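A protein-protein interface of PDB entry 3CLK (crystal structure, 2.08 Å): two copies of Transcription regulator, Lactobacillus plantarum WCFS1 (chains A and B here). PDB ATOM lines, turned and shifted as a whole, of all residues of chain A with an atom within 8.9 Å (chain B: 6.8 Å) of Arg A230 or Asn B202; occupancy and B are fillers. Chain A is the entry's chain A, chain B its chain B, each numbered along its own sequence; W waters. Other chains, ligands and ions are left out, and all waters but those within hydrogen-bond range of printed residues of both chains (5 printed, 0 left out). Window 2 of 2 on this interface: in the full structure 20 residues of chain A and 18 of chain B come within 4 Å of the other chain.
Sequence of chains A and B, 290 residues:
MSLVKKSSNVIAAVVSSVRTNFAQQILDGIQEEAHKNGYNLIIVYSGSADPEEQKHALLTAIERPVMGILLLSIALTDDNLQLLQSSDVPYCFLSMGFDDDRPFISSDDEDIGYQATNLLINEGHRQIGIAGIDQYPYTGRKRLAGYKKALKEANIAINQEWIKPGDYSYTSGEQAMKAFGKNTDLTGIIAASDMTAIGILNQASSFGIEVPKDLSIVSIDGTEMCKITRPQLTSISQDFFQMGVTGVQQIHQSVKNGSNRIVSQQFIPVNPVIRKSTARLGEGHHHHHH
The side-chain amide nitrogen (ND2) of Asn A202 lies close to the guanidinium group (NH2) of Arg B230, at 3.4 Å. The backbone carbonyl oxygen (O) of Ile A228 sits at hydrogen-bond distance from the side-chain amide nitrogen (ND2) of Asn B202, at 2.8 Å.
NH1 of Arg A230 sits at hydrogen-bond distance from O of Lys A227. OE2 of Glu B174 lies close to OH of Tyr B170, 3.5 Å away. ND2 of Asn B202 lies within hydrogen-bond range of OH of Tyr B170 (2.8 Å). The side-chain hydroxyl of Ser B206 is in hydrogen-bond range of the backbone carbonyl oxygen of Asn B202 (3.3 Å).
CG2 of Ile A228 touches CE1 of Tyr B170, at 3.5 Å. O of Ile A228 touches CG2 of Ile B198, at 3.996 Å. Arg A230 touches Tyr B170. OD1 of Asn B202 touches CG of Arg A230 (3.6 Å).
Arg A230 touches just these residues of chain B: Tyr B170 (3.6 Å) and Asn B202 (3.6 Å). Of the printed residues of chain A, Tyr B170 touches Ile A228 (3.5 Å) and Arg A230 (3.6 Å). No residue of chain A comes within 4 Å of Gly B199. Of the printed residues of chain A, Arg B230 touches Asn A202. The nearest residue of chain A that does not touch Asn B202 is Thr A229 (4.8 Å).
Of the 19 printed residues of chain A, 3 touch a printed residue of chain B. Of the 17 printed residues of chain B, 4 touch a printed residue of chain A. Among the printed residues, 6 pairs touch across the chains. Among the printed residues, no Asp or Glu carboxylate lies within 4 Å of a Lys or Arg side-chain nitrogen of the other chain.
Asn A202 touches Arg B230, and with the chains exchanged Arg A230 touches Asn B202. Positions printed for both chains: 198, 201, 202, 205, 229 and 230. Of the 6 pairs that touch across the chains among the printed residues, 2 have their exchanged pair printed and touching as well.
Water W3 bridges O of Asn A202 and NH1 of Arg B230. Water W4 bridges NH1 of Arg B230 (2.6 Å) and O of Asn A202 (3.2 Å). Water W5 lies within hydrogen-bond range of the side-chain carboxylate of Glu B174 (2.6 Å), the side-chain hydroxyl of Tyr B170 (2.8 Å) and the guanidinium group of Arg A230 (2.9 Å). Water W1 lies within hydrogen-bond range of the side-chain hydroxyl of Ser B206, the guanidinium group of Arg A230 and the backbone carbonyl oxygen of Asn B202. Water W2 lies within hydrogen-bond range of O of Asn B202, NE of Arg A230 and OG of Ser B206.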
ATOM      1  N   ILE A 198     -36.945   5.464  -8.311  1.00  0.00           N
ATOM      2  CA  ILE A 198     -36.113   6.630  -8.027  1.00  0.00           C
ATOM      3  C   ILE A 198     -36.673   7.398  -6.835  1.00  0.00           C
ATOM      4  O   ILE A 198     -35.919   7.921  -6.020  1.00  0.00           O
ATOM      5  CB  ILE A 198     -36.030   7.567  -9.253  1.00  0.00           C
ATOM      6  CG1 ILE A 198     -35.404   6.814 -10.427  1.00  0.00           C
ATOM      7  CG2 ILE A 198     -35.186   8.795  -8.921  1.00  0.00           C
ATOM      8  CD1 ILE A 198     -35.418   7.588 -11.719  1.00  0.00           C
ATOM      9  N   LEU A 201     -35.598   5.475  -3.841  1.00  0.00           N
ATOM     10  CA  LEU A 201     -34.164   5.649  -3.644  1.00  0.00           C
ATOM     11  C   LEU A 201     -33.823   7.009  -3.037  1.00  0.00           C
ATOM     12  O   LEU A 201     -33.031   7.085  -2.097  1.00  0.00           O
ATOM     13  CB  LEU A 201     -33.428   5.501  -4.972  1.00  0.00           C
ATOM     14  CG  LEU A 201     -31.935   5.832  -4.980  1.00  0.00           C
ATOM     15  CD1 LEU A 201     -31.185   4.791  -4.168  1.00  0.00           C
ATOM     16  CD2 LEU A 201     -31.421   5.841  -6.423  1.00  0.00           C
ATOM     17  N   ASN A 202     -34.412   8.078  -3.571  1.00  0.00           N
ATOM     18  CA  ASN A 202     -34.124   9.414  -3.054  1.00  0.00           C
ATOM     19  C   ASN A 202     -34.644   9.627  -1.634  1.00  0.00           C
ATOM     20  O   ASN A 202     -33.943  10.200  -0.798  1.00  0.00           O
ATOM     21  CB  ASN A 202     -34.678  10.494  -4.001  1.00  0.00           C
ATOM     22  CG  ASN A 202     -33.895  10.575  -5.313  1.00  0.00           C
ATOM     23  OD1 ASN A 202     -32.882   9.906  -5.481  1.00  0.00           O
ATOM     24  ND2 ASN A 202     -34.363  11.402  -6.238  1.00  0.00           N
ATOM     25  N   SER A 205     -32.555   7.690   0.865  1.00  0.00           N
ATOM     26  CA  SER A 205     -31.304   8.394   1.085  1.00  0.00           C
ATOM     27  C   SER A 205     -31.463   9.598   2.010  1.00  0.00           C
ATOM     28  O   SER A 205     -30.597   9.868   2.842  1.00  0.00           O
ATOM     29  CB  SER A 205     -30.717   8.854  -0.243  1.00  0.00           C
ATOM     30  OG  SER A 205     -29.619   9.710  -0.014  1.00  0.00           O
ATOM     31  N   VAL A 211     -28.298   2.623  -0.097  1.00  0.00           N
ATOM     32  CA  VAL A 211     -28.671   1.588  -1.051  1.00  0.00           C
ATOM     33  C   VAL A 211     -27.411   1.235  -1.829  1.00  0.00           C
ATOM     34  O   VAL A 211     -26.765   2.117  -2.391  1.00  0.00           O
ATOM     35  CB  VAL A 211     -29.742   2.104  -2.047  1.00  0.00           C
ATOM     36  CG1 VAL A 211     -29.946   1.090  -3.178  1.00  0.00           C
ATOM     37  CG2 VAL A 211     -31.055   2.362  -1.310  1.00  0.00           C
ATOM     38  N   PRO A 212     -27.071  -0.061  -1.919  1.00  0.00           N
ATOM     39  CA  PRO A 212     -27.774  -1.222  -1.371  1.00  0.00           C
ATOM     40  C   PRO A 212     -27.295  -1.699   0.005  1.00  0.00           C
ATOM     41  O   PRO A 212     -27.764  -2.720   0.504  1.00  0.00           O
ATOM     42  CB  PRO A 212     -27.530  -2.275  -2.436  1.00  0.00           C
ATOM     43  CG  PRO A 212     -26.052  -2.025  -2.735  1.00  0.00           C
ATOM     44  CD  PRO A 212     -25.968  -0.497  -2.803  1.00  0.00           C
ATOM     45  N   GLU A 224     -33.807   3.618 -19.596  1.00  0.00           N
ATOM     46  CA  GLU A 224     -32.550   4.327 -19.370  1.00  0.00           C
ATOM     47  C   GLU A 224     -32.523   5.050 -18.031  1.00  0.00           C
ATOM     48  O   GLU A 224     -31.449   5.352 -17.513  1.00  0.00           O
ATOM     49  CB  GLU A 224     -32.301   5.327 -20.498  1.00  0.00           C
ATOM     50  CG  GLU A 224     -32.225   4.668 -21.864  1.00  0.00           C
ATOM     51  CD  GLU A 224     -31.102   3.652 -21.961  1.00  0.00           C
ATOM     52  OE1 GLU A 224     -29.920   4.063 -21.917  1.00  0.00           O
ATOM     53  OE2 GLU A 224     -31.404   2.440 -22.081  1.00  0.00           O
ATOM     54  N   MET A 225     -33.699   5.343 -17.480  1.00  0.00           N
ATOM     55  CA  MET A 225     -33.780   6.002 -16.176  1.00  0.00           C
ATOM     56  C   MET A 225     -32.917   5.223 -15.172  1.00  0.00           C
ATOM     57  O   MET A 225     -32.272   5.808 -14.295  1.00  0.00           O
ATOM     58  CB  MET A 225     -35.235   6.037 -15.662  1.00  0.00           C
ATOM     59  CG  MET A 225     -36.163   7.042 -16.349  1.00  0.00           C
ATOM     60  SD  MET A 225     -35.544   8.912 -16.176  1.00  0.00           S
ATOM     61  CE  MET A 225     -34.478   8.968 -17.775  1.00  0.00           C
ATOM     62  N   CYS A 226     -32.903   3.899 -15.300  1.00  0.00           N
ATOM     63  CA  CYS A 226     -32.124   3.074 -14.382  1.00  0.00           C
ATOM     64  C   CYS A 226     -30.624   3.307 -14.503  1.00  0.00           C
ATOM     65  O   CYS A 226     -29.882   3.061 -13.560  1.00  0.00           O
ATOM     66  CB  CYS A 226     -32.414   1.587 -14.616  1.00  0.00           C
ATOM     67  SG  CYS A 226     -34.104   1.094 -14.224  1.00  0.00           S
ATOM     68  N   LYS A 227     -30.187   3.795 -15.662  1.00  0.00           N
ATOM     69  CA  LYS A 227     -28.771   4.023 -15.908  1.00  0.00           C
ATOM     70  C   LYS A 227     -28.237   5.371 -15.468  1.00  0.00           C
ATOM     71  O   LYS A 227     -27.026   5.531 -15.288  1.00  0.00           O
ATOM     72  CB  LYS A 227     -28.466   3.834 -17.395  1.00  0.00           C
ATOM     73  CG  LYS A 227     -28.636   2.397 -17.878  1.00  0.00           C
ATOM     74  CD  LYS A 227     -28.330   2.273 -19.366  1.00  0.00           C
ATOM     75  CE  LYS A 227     -28.507   0.840 -19.843  1.00  0.00           C
ATOM     76  NZ  LYS A 227     -27.649  -0.121 -19.087  1.00  0.00           N
ATOM     77  N   ILE A 228     -29.120   6.345 -15.292  1.00  0.00           N
ATOM     78  CA  ILE A 228     -28.670   7.669 -14.899  1.00  0.00           C
ATOM     79  C   ILE A 228     -28.804   7.929 -13.412  1.00  0.00           C
ATOM     80  O   ILE A 228     -28.435   8.999 -12.931  1.00  0.00           O
ATOM     81  CB  ILE A 228     -29.417   8.753 -15.683  1.00  0.00           C
ATOM     82  CG1 ILE A 228     -30.875   8.821 -15.240  1.00  0.00           C
ATOM     83  CG2 ILE A 228     -29.343   8.430 -17.169  1.00  0.00           C
ATOM     84  CD1 ILE A 228     -31.628   9.969 -15.860  1.00  0.00           C
ATOM     85  N   THR A 229     -29.339   6.956 -12.674  1.00  0.00           N
ATOM     86  CA  THR A 229     -29.463   7.121 -11.234  1.00  0.00           C
ATOM     87  C   THR A 229     -28.184   6.575 -10.621  1.00  0.00           C
ATOM     88  O   THR A 229     -27.442   5.837 -11.270  1.00  0.00           O
ATOM     89  CB  THR A 229     -30.649   6.338 -10.656  1.00  0.00           C
ATOM     90  OG1 THR A 229     -30.443   4.931 -10.874  1.00  0.00           O
ATOM     91  CG2 THR A 229     -31.946   6.790 -11.305  1.00  0.00           C
ATOM     92  N   ARG A 230     -27.919   6.956  -9.379  1.00  0.00           N
ATOM     93  CA  ARG A 230     -26.732   6.498  -8.673  1.00  0.00           C
ATOM     94  C   ARG A 230     -27.169   6.132  -7.264  1.00  0.00           C
ATOM     95  O   ARG A 230     -27.618   6.994  -6.502  1.00  0.00           O
ATOM     96  CB  ARG A 230     -25.675   7.609  -8.619  1.00  0.00           C
ATOM     97  CG  ARG A 230     -25.074   7.966  -9.974  1.00  0.00           C
ATOM     98  CD  ARG A 230     -24.179   6.840 -10.480  1.00  0.00           C
ATOM     99  NE  ARG A 230     -23.549   7.180 -11.754  1.00  0.00           N
ATOM    100  CZ  ARG A 230     -24.104   7.000 -12.947  1.00  0.00           C
ATOM    101  NH1 ARG A 230     -25.317   6.475 -13.055  1.00  0.00           N
ATOM    102  NH2 ARG A 230     -23.440   7.350 -14.043  1.00  0.00           N
ATOM    103  N   PRO A 231     -27.082   4.841  -6.910  1.00  0.00           N
ATOM    104  CA  PRO A 231     -26.602   3.749  -7.766  1.00  0.00           C
ATOM    105  C   PRO A 231     -27.564   3.397  -8.902  1.00  0.00           C
ATOM    106  O   PRO A 231     -28.777   3.623  -8.800  1.00  0.00           O
ATOM    107  CB  PRO A 231     -26.459   2.594  -6.785  1.00  0.00           C
ATOM    108  CG  PRO A 231     -27.643   2.820  -5.881  1.00  0.00           C
ATOM    109  CD  PRO A 231     -27.523   4.317  -5.603  1.00  0.00           C
ATOM    110  N   GLN A 232     -27.020   2.836  -9.978  1.00  0.00           N
ATOM    111  CA  GLN A 232     -27.843   2.429 -11.102  1.00  0.00           C
ATOM    112  C   GLN A 232     -28.807   1.360 -10.593  1.00  0.00           C
ATOM    113  O   GLN A 232     -28.434   0.499  -9.793  1.00  0.00           O
ATOM    114  CB  GLN A 232     -26.971   1.903 -12.243  1.00  0.00           C
ATOM    115  CG  GLN A 232     -26.063   2.994 -12.830  1.00  0.00           C
ATOM    116  CD  GLN A 232     -25.416   2.608 -14.151  1.00  0.00           C
ATOM    117  OE1 GLN A 232     -24.602   3.355 -14.692  1.00  0.00           O
ATOM    118  NE2 GLN A 232     -25.781   1.442 -14.679  1.00  0.00           N
ATOM    119  N   LEU A 233     -30.049   1.430 -11.061  1.00  0.00           N
ATOM    120  CA  LEU A 233     -31.098   0.525 -10.620  1.00  0.00           C
ATOM    121  C   LEU A 233     -31.213  -0.846 -11.270  1.00  0.00           C
ATOM    122  O   LEU A 233     -31.382  -0.962 -12.491  1.00  0.00           O
ATOM    123  CB  LEU A 233     -32.459   1.224 -10.743  1.00  0.00           C
ATOM    124  CG  LEU A 233     -32.687   2.454  -9.857  1.00  0.00           C
ATOM    125  CD1 LEU A 233     -33.956   3.183 -10.302  1.00  0.00           C
ATOM    126  CD2 LEU A 233     -32.795   2.015  -8.394  1.00  0.00           C
ATOM    127  N   ARG A 275     -27.707  -4.319 -11.744  1.00  0.00           N
ATOM    128  CA  ARG A 275     -26.904  -3.109 -11.718  1.00  0.00           C
ATOM    129  C   ARG A 275     -26.280  -2.915 -10.345  1.00  0.00           C
ATOM    130  O   ARG A 275     -25.577  -3.800  -9.862  1.00  0.00           O
ATOM    131  CB  ARG A 275     -27.728  -1.886 -12.152  1.00  0.00           C
ATOM    132  CG  ARG A 275     -28.247  -2.025 -13.585  1.00  0.00           C
ATOM    133  CD  ARG A 275     -28.670  -0.706 -14.238  1.00  0.00           C
ATOM    134  NE  ARG A 275     -29.071  -0.933 -15.631  1.00  0.00           N
ATOM    135  CZ  ARG A 275     -30.251  -1.429 -16.003  1.00  0.00           C
ATOM    136  NH1 ARG A 275     -31.168  -1.741 -15.096  1.00  0.00           N
ATOM    137  NH2 ARG A 275     -30.505  -1.652 -17.281  1.00  0.00           N
ATOM    138  N   LYS A 276     -26.543  -1.791  -9.692  1.00  0.00           N
ATOM    139  CA  LYS A 276     -25.903  -1.552  -8.404  1.00  0.00           C
ATOM    140  C   LYS A 276     -26.821  -1.282  -7.232  1.00  0.00           C
ATOM    141  O   LYS A 276     -26.347  -0.854  -6.178  1.00  0.00           O
ATOM    142  CB  LYS A 276     -24.937  -0.372  -8.546  1.00  0.00           C
ATOM    143  CG  LYS A 276     -23.837  -0.601  -9.574  1.00  0.00           C
ATOM    144  CD  LYS A 276     -22.824  -1.600  -9.050  1.00  0.00           C
ATOM    145  CE  LYS A 276     -21.816  -1.979 -10.126  1.00  0.00           C
ATOM    146  NZ  LYS A 276     -21.248  -0.775 -10.789  1.00  0.00           N
ATOM    147  N   SER A 277     -28.119  -1.527  -7.394  1.00  0.00           N
ATOM    148  CA  SER A 277     -29.059  -1.243  -6.311  1.00  0.00           C
ATOM    149  C   SER A 277     -29.514  -2.427  -5.448  1.00  0.00           C
ATOM    150  O   SER A 277     -30.447  -2.283  -4.654  1.00  0.00           O
ATOM    151  CB  SER A 277     -30.291  -0.515  -6.866  1.00  0.00           C
ATOM    152  OG  SER A 277     -31.025  -1.345  -7.754  1.00  0.00           O
ATOM    153  N   TYR B 170     -28.015  13.469 -22.415  1.00  0.00           N
ATOM    154  CA  TYR B 170     -27.360  13.059 -21.184  1.00  0.00           C
ATOM    155  C   TYR B 170     -25.893  12.742 -21.495  1.00  0.00           C
ATOM    156  O   TYR B 170     -24.989  13.141 -20.758  1.00  0.00           O
ATOM    157  CB  TYR B 170     -28.050  11.816 -20.631  1.00  0.00           C
ATOM    158  CG  TYR B 170     -27.342  11.185 -19.460  1.00  0.00           C
ATOM    159  CD1 TYR B 170     -27.555  11.645 -18.163  1.00  0.00           C
ATOM    160  CD2 TYR B 170     -26.489  10.098 -19.645  1.00  0.00           C
ATOM    161  CE1 TYR B 170     -26.944  11.029 -17.073  1.00  0.00           C
ATOM    162  CE2 TYR B 170     -25.870   9.477 -18.558  1.00  0.00           C
ATOM    163  CZ  TYR B 170     -26.106   9.949 -17.279  1.00  0.00           C
ATOM    164  OH  TYR B 170     -25.509   9.328 -16.205  1.00  0.00           O
ATOM    165  N   GLU B 174     -22.085  14.031 -19.929  1.00  0.00           N
ATOM    166  CA  GLU B 174     -20.982  13.216 -19.440  1.00  0.00           C
ATOM    167  C   GLU B 174     -19.703  13.508 -20.221  1.00  0.00           C
ATOM    168  O   GLU B 174     -18.613  13.602 -19.635  1.00  0.00           O
ATOM    169  CB  GLU B 174     -21.284  11.729 -19.598  1.00  0.00           C
ATOM    170  CG  GLU B 174     -22.426  11.176 -18.770  1.00  0.00           C
ATOM    171  CD  GLU B 174     -22.557   9.679 -18.993  1.00  0.00           C
ATOM    172  OE1 GLU B 174     -22.638   9.271 -20.171  1.00  0.00           O
ATOM    173  OE2 GLU B 174     -22.570   8.917 -18.011  1.00  0.00           O
ATOM    174  N   MET B 177     -18.159  16.932 -19.374  1.00  0.00           N
ATOM    175  CA  MET B 177     -17.501  16.963 -18.060  1.00  0.00           C
ATOM    176  C   MET B 177     -16.121  16.288 -18.163  1.00  0.00           C
ATOM    177  O   MET B 177     -15.156  16.712 -17.512  1.00  0.00           O
ATOM    178  CB  MET B 177     -18.379  16.286 -16.997  1.00  0.00           C
ATOM    179  CG  MET B 177     -17.835  16.363 -15.558  1.00  0.00           C
ATOM    180  SD  MET B 177     -17.627  18.188 -14.861  1.00  0.00           S
ATOM    181  CE  MET B 177     -15.689  18.299 -14.711  1.00  0.00           C
ATOM    182  N   ALA B 197     -27.526  18.131 -17.716  1.00  0.00           N
ATOM    183  CA  ALA B 197     -27.094  18.421 -16.355  1.00  0.00           C
ATOM    184  C   ALA B 197     -26.892  17.142 -15.550  1.00  0.00           C
ATOM    185  O   ALA B 197     -25.972  17.044 -14.738  1.00  0.00           O
ATOM    186  CB  ALA B 197     -28.120  19.304 -15.668  1.00  0.00           C
ATOM    187  N   ILE B 198     -27.742  16.149 -15.767  1.00  0.00           N
ATOM    188  CA  ILE B 198     -27.591  14.922 -15.014  1.00  0.00           C
ATOM    189  C   ILE B 198     -26.289  14.235 -15.423  1.00  0.00           C
ATOM    190  O   ILE B 198     -25.585  13.700 -14.573  1.00  0.00           O
ATOM    191  CB  ILE B 198     -28.808  13.989 -15.208  1.00  0.00           C
ATOM    192  CG1 ILE B 198     -30.085  14.704 -14.758  1.00  0.00           C
ATOM    193  CG2 ILE B 198     -28.651  12.730 -14.346  1.00  0.00           C
ATOM    194  CD1 ILE B 198     -31.330  13.859 -14.895  1.00  0.00           C
ATOM    195  N   GLY B 199     -25.954  14.280 -16.714  1.00  0.00           N
ATOM    196  CA  GLY B 199     -24.715  13.669 -17.179  1.00  0.00           C
ATOM    197  C   GLY B 199     -23.507  14.367 -16.564  1.00  0.00           C
ATOM    198  O   GLY B 199     -22.538  13.730 -16.137  1.00  0.00           O
ATOM    199  N   ILE B 200     -23.559  15.692 -16.521  1.00  0.00           N
ATOM    200  CA  ILE B 200     -22.481  16.479 -15.930  1.00  0.00           C
ATOM    201  C   ILE B 200     -22.360  16.087 -14.464  1.00  0.00           C
ATOM    202  O   ILE B 200     -21.264  15.829 -13.959  1.00  0.00           O
ATOM    203  CB  ILE B 200     -22.793  17.991 -15.991  1.00  0.00           C
ATOM    204  CG1 ILE B 200     -22.783  18.467 -17.442  1.00  0.00           C
ATOM    205  CG2 ILE B 200     -21.775  18.779 -15.147  1.00  0.00           C
ATOM    206  CD1 ILE B 200     -23.312  19.878 -17.626  1.00  0.00           C
ATOM    207  N   LEU B 201     -23.506  16.046 -13.792  1.00  0.00           N
ATOM    208  CA  LEU B 201     -23.592  15.712 -12.375  1.00  0.00           C
ATOM    209  C   LEU B 201     -22.992  14.357 -12.041  1.00  0.00           C
ATOM    210  O   LEU B 201     -22.217  14.222 -11.080  1.00  0.00           O
ATOM    211  CB  LEU B 201     -25.060  15.729 -11.932  1.00  0.00           C
ATOM    212  CG  LEU B 201     -25.385  15.773 -10.431  1.00  0.00           C
ATOM    213  CD1 LEU B 201     -26.909  15.760 -10.223  1.00  0.00           C
ATOM    214  CD2 LEU B 201     -24.768  14.594  -9.735  1.00  0.00           C
ATOM    215  N   ASN B 202     -23.371  13.343 -12.811  1.00  0.00           N
ATOM    216  CA  ASN B 202     -22.870  12.004 -12.569  1.00  0.00           C
ATOM    217  C   ASN B 202     -21.383  11.884 -12.897  1.00  0.00           C
ATOM    218  O   ASN B 202     -20.648  11.236 -12.154  1.00  0.00           O
ATOM    219  CB  ASN B 202     -23.674  10.971 -13.371  1.00  0.00           C
ATOM    220  CG  ASN B 202     -25.082  10.761 -12.818  1.00  0.00           C
ATOM    221  OD1 ASN B 202     -25.378  11.128 -11.676  1.00  0.00           O
ATOM    222  ND2 ASN B 202     -25.948  10.155 -13.619  1.00  0.00           N
ATOM    223  N   GLN B 203     -20.935  12.498 -13.995  1.00  0.00           N
ATOM    224  CA  GLN B 203     -19.521  12.415 -14.354  1.00  0.00           C
ATOM    225  C   GLN B 203     -18.667  13.145 -13.332  1.00  0.00           C
ATOM    226  O   GLN B 203     -17.587  12.679 -12.975  1.00  0.00           O
ATOM    227  CB  GLN B 203     -19.240  12.989 -15.748  1.00  0.00           C
ATOM    228  CG  GLN B 203     -17.774  12.780 -16.191  1.00  0.00           C
ATOM    229  CD  GLN B 203     -17.381  11.305 -16.235  1.00  0.00           C
ATOM    230  OE1 GLN B 203     -16.262  10.928 -15.871  1.00  0.00           O
ATOM    231  NE2 GLN B 203     -18.299  10.469 -16.686  1.00  0.00           N
ATOM    232  N   ALA B 204     -19.143  14.297 -12.871  1.00  0.00           N
ATOM    233  CA  ALA B 204     -18.406  15.055 -11.858  1.00  0.00           C
ATOM    234  C   ALA B 204     -18.249  14.146 -10.645  1.00  0.00           C
ATOM    235  O   ALA B 204     -17.169  14.033 -10.065  1.00  0.00           O
ATOM    236  CB  ALA B 204     -19.181  16.306 -11.463  1.00  0.00           C
ATOM    237  N   SER B 205     -19.338  13.489 -10.273  1.00  0.00           N
ATOM    238  CA  SER B 205     -19.337  12.587  -9.134  1.00  0.00           C
ATOM    239  C   SER B 205     -18.282  11.494  -9.300  1.00  0.00           C
ATOM    240  O   SER B 205     -17.557  11.167  -8.356  1.00  0.00           O
ATOM    241  CB  SER B 205     -20.723  11.973  -8.961  1.00  0.00           C
ATOM    242  OG  SER B 205     -20.750  11.120  -7.834  1.00  0.00           O
ATOM    243  N   SER B 206     -18.185  10.937 -10.503  1.00  0.00           N
ATOM    244  CA  SER B 206     -17.203   9.900 -10.782  1.00  0.00           C
ATOM    245  C   SER B 206     -15.772  10.426 -10.642  1.00  0.00           C
ATOM    246  O   SER B 206     -14.855   9.666 -10.308  1.00  0.00           O
ATOM    247  CB  SER B 206     -17.414   9.331 -12.185  1.00  0.00           C
ATOM    248  OG  SER B 206     -18.650   8.633 -12.259  1.00  0.00           O
ATOM    249  N   PHE B 207     -15.581  11.716 -10.906  1.00  0.00           N
ATOM    250  CA  PHE B 207     -14.260  12.332 -10.779  1.00  0.00           C
ATOM    251  C   PHE B 207     -13.994  12.723  -9.316  1.00  0.00           C
ATOM    252  O   PHE B 207     -12.926  13.241  -8.987  1.00  0.00           O
ATOM    253  CB  PHE B 207     -14.153  13.594 -11.656  1.00  0.00           C
ATOM    254  CG  PHE B 207     -13.922  13.322 -13.129  1.00  0.00           C
ATOM    255  CD1 PHE B 207     -13.306  12.155 -13.557  1.00  0.00           C
ATOM    256  CD2 PHE B 207     -14.258  14.286 -14.083  1.00  0.00           C
ATOM    257  CE1 PHE B 207     -13.022  11.946 -14.911  1.00  0.00           C
ATOM    258  CE2 PHE B 207     -13.977  14.088 -15.440  1.00  0.00           C
ATOM    259  CZ  PHE B 207     -13.357  12.914 -15.852  1.00  0.00           C
ATOM    260  N   ILE B 217     -23.902  23.642 -10.485  1.00  0.00           N
ATOM    261  CA  ILE B 217     -24.490  23.311 -11.782  1.00  0.00           C
ATOM    262  C   ILE B 217     -25.860  23.957 -11.904  1.00  0.00           C
ATOM    263  O   ILE B 217     -26.675  23.842 -10.999  1.00  0.00           O
ATOM    264  CB  ILE B 217     -24.681  21.785 -11.968  1.00  0.00           C
ATOM    265  CG1 ILE B 217     -23.327  21.073 -11.954  1.00  0.00           C
ATOM    266  CG2 ILE B 217     -25.428  21.520 -13.276  1.00  0.00           C
ATOM    267  CD1 ILE B 217     -23.434  19.558 -12.019  1.00  0.00           C
ATOM    268  N   THR B 229     -32.644  14.013  -9.195  1.00  0.00           N
ATOM    269  CA  THR B 229     -31.220  13.775  -8.988  1.00  0.00           C
ATOM    270  C   THR B 229     -30.827  14.240  -7.593  1.00  0.00           C
ATOM    271  O   THR B 229     -31.550  15.003  -6.960  1.00  0.00           O
ATOM    272  CB  THR B 229     -30.359  14.538 -10.010  1.00  0.00           C
ATOM    273  OG1 THR B 229     -30.627  15.945  -9.908  1.00  0.00           O
ATOM    274  CG2 THR B 229     -30.670  14.069 -11.416  1.00  0.00           C
ATOM    275  N   ARG B 230     -29.687  13.764  -7.116  1.00  0.00           N
ATOM    276  CA  ARG B 230     -29.178  14.153  -5.806  1.00  0.00           C
ATOM    277  C   ARG B 230     -27.776  14.720  -6.005  1.00  0.00           C
ATOM    278  O   ARG B 230     -26.853  13.989  -6.354  1.00  0.00           O
ATOM    279  CB  ARG B 230     -29.105  12.946  -4.867  1.00  0.00           C
ATOM    280  CG  ARG B 230     -30.452  12.354  -4.486  1.00  0.00           C
ATOM    281  CD  ARG B 230     -31.346  13.348  -3.749  1.00  0.00           C
ATOM    282  NE  ARG B 230     -32.343  13.929  -4.643  1.00  0.00           N
ATOM    283  CZ  ARG B 230     -33.605  14.171  -4.305  1.00  0.00           C
ATOM    284  NH1 ARG B 230     -34.039  13.891  -3.084  1.00  0.00           N
ATOM    285  NH2 ARG B 230     -34.443  14.672  -5.198  1.00  0.00           N
HETATM  286  O   HOH W   1     -20.789   8.262 -13.897  1.00  0.00           O
HETATM  287  O   HOH W   2     -21.391   8.877 -11.017  1.00  0.00           O
HETATM  288  O   HOH W   3     -32.478  12.265  -1.075  1.00  0.00           O
HETATM  289  O   HOH W   4     -35.158  13.144  -0.858  1.00  0.00           O
HETATM  290  O   HOH W   5     -24.092   7.061 -16.892  1.00  0.00           O
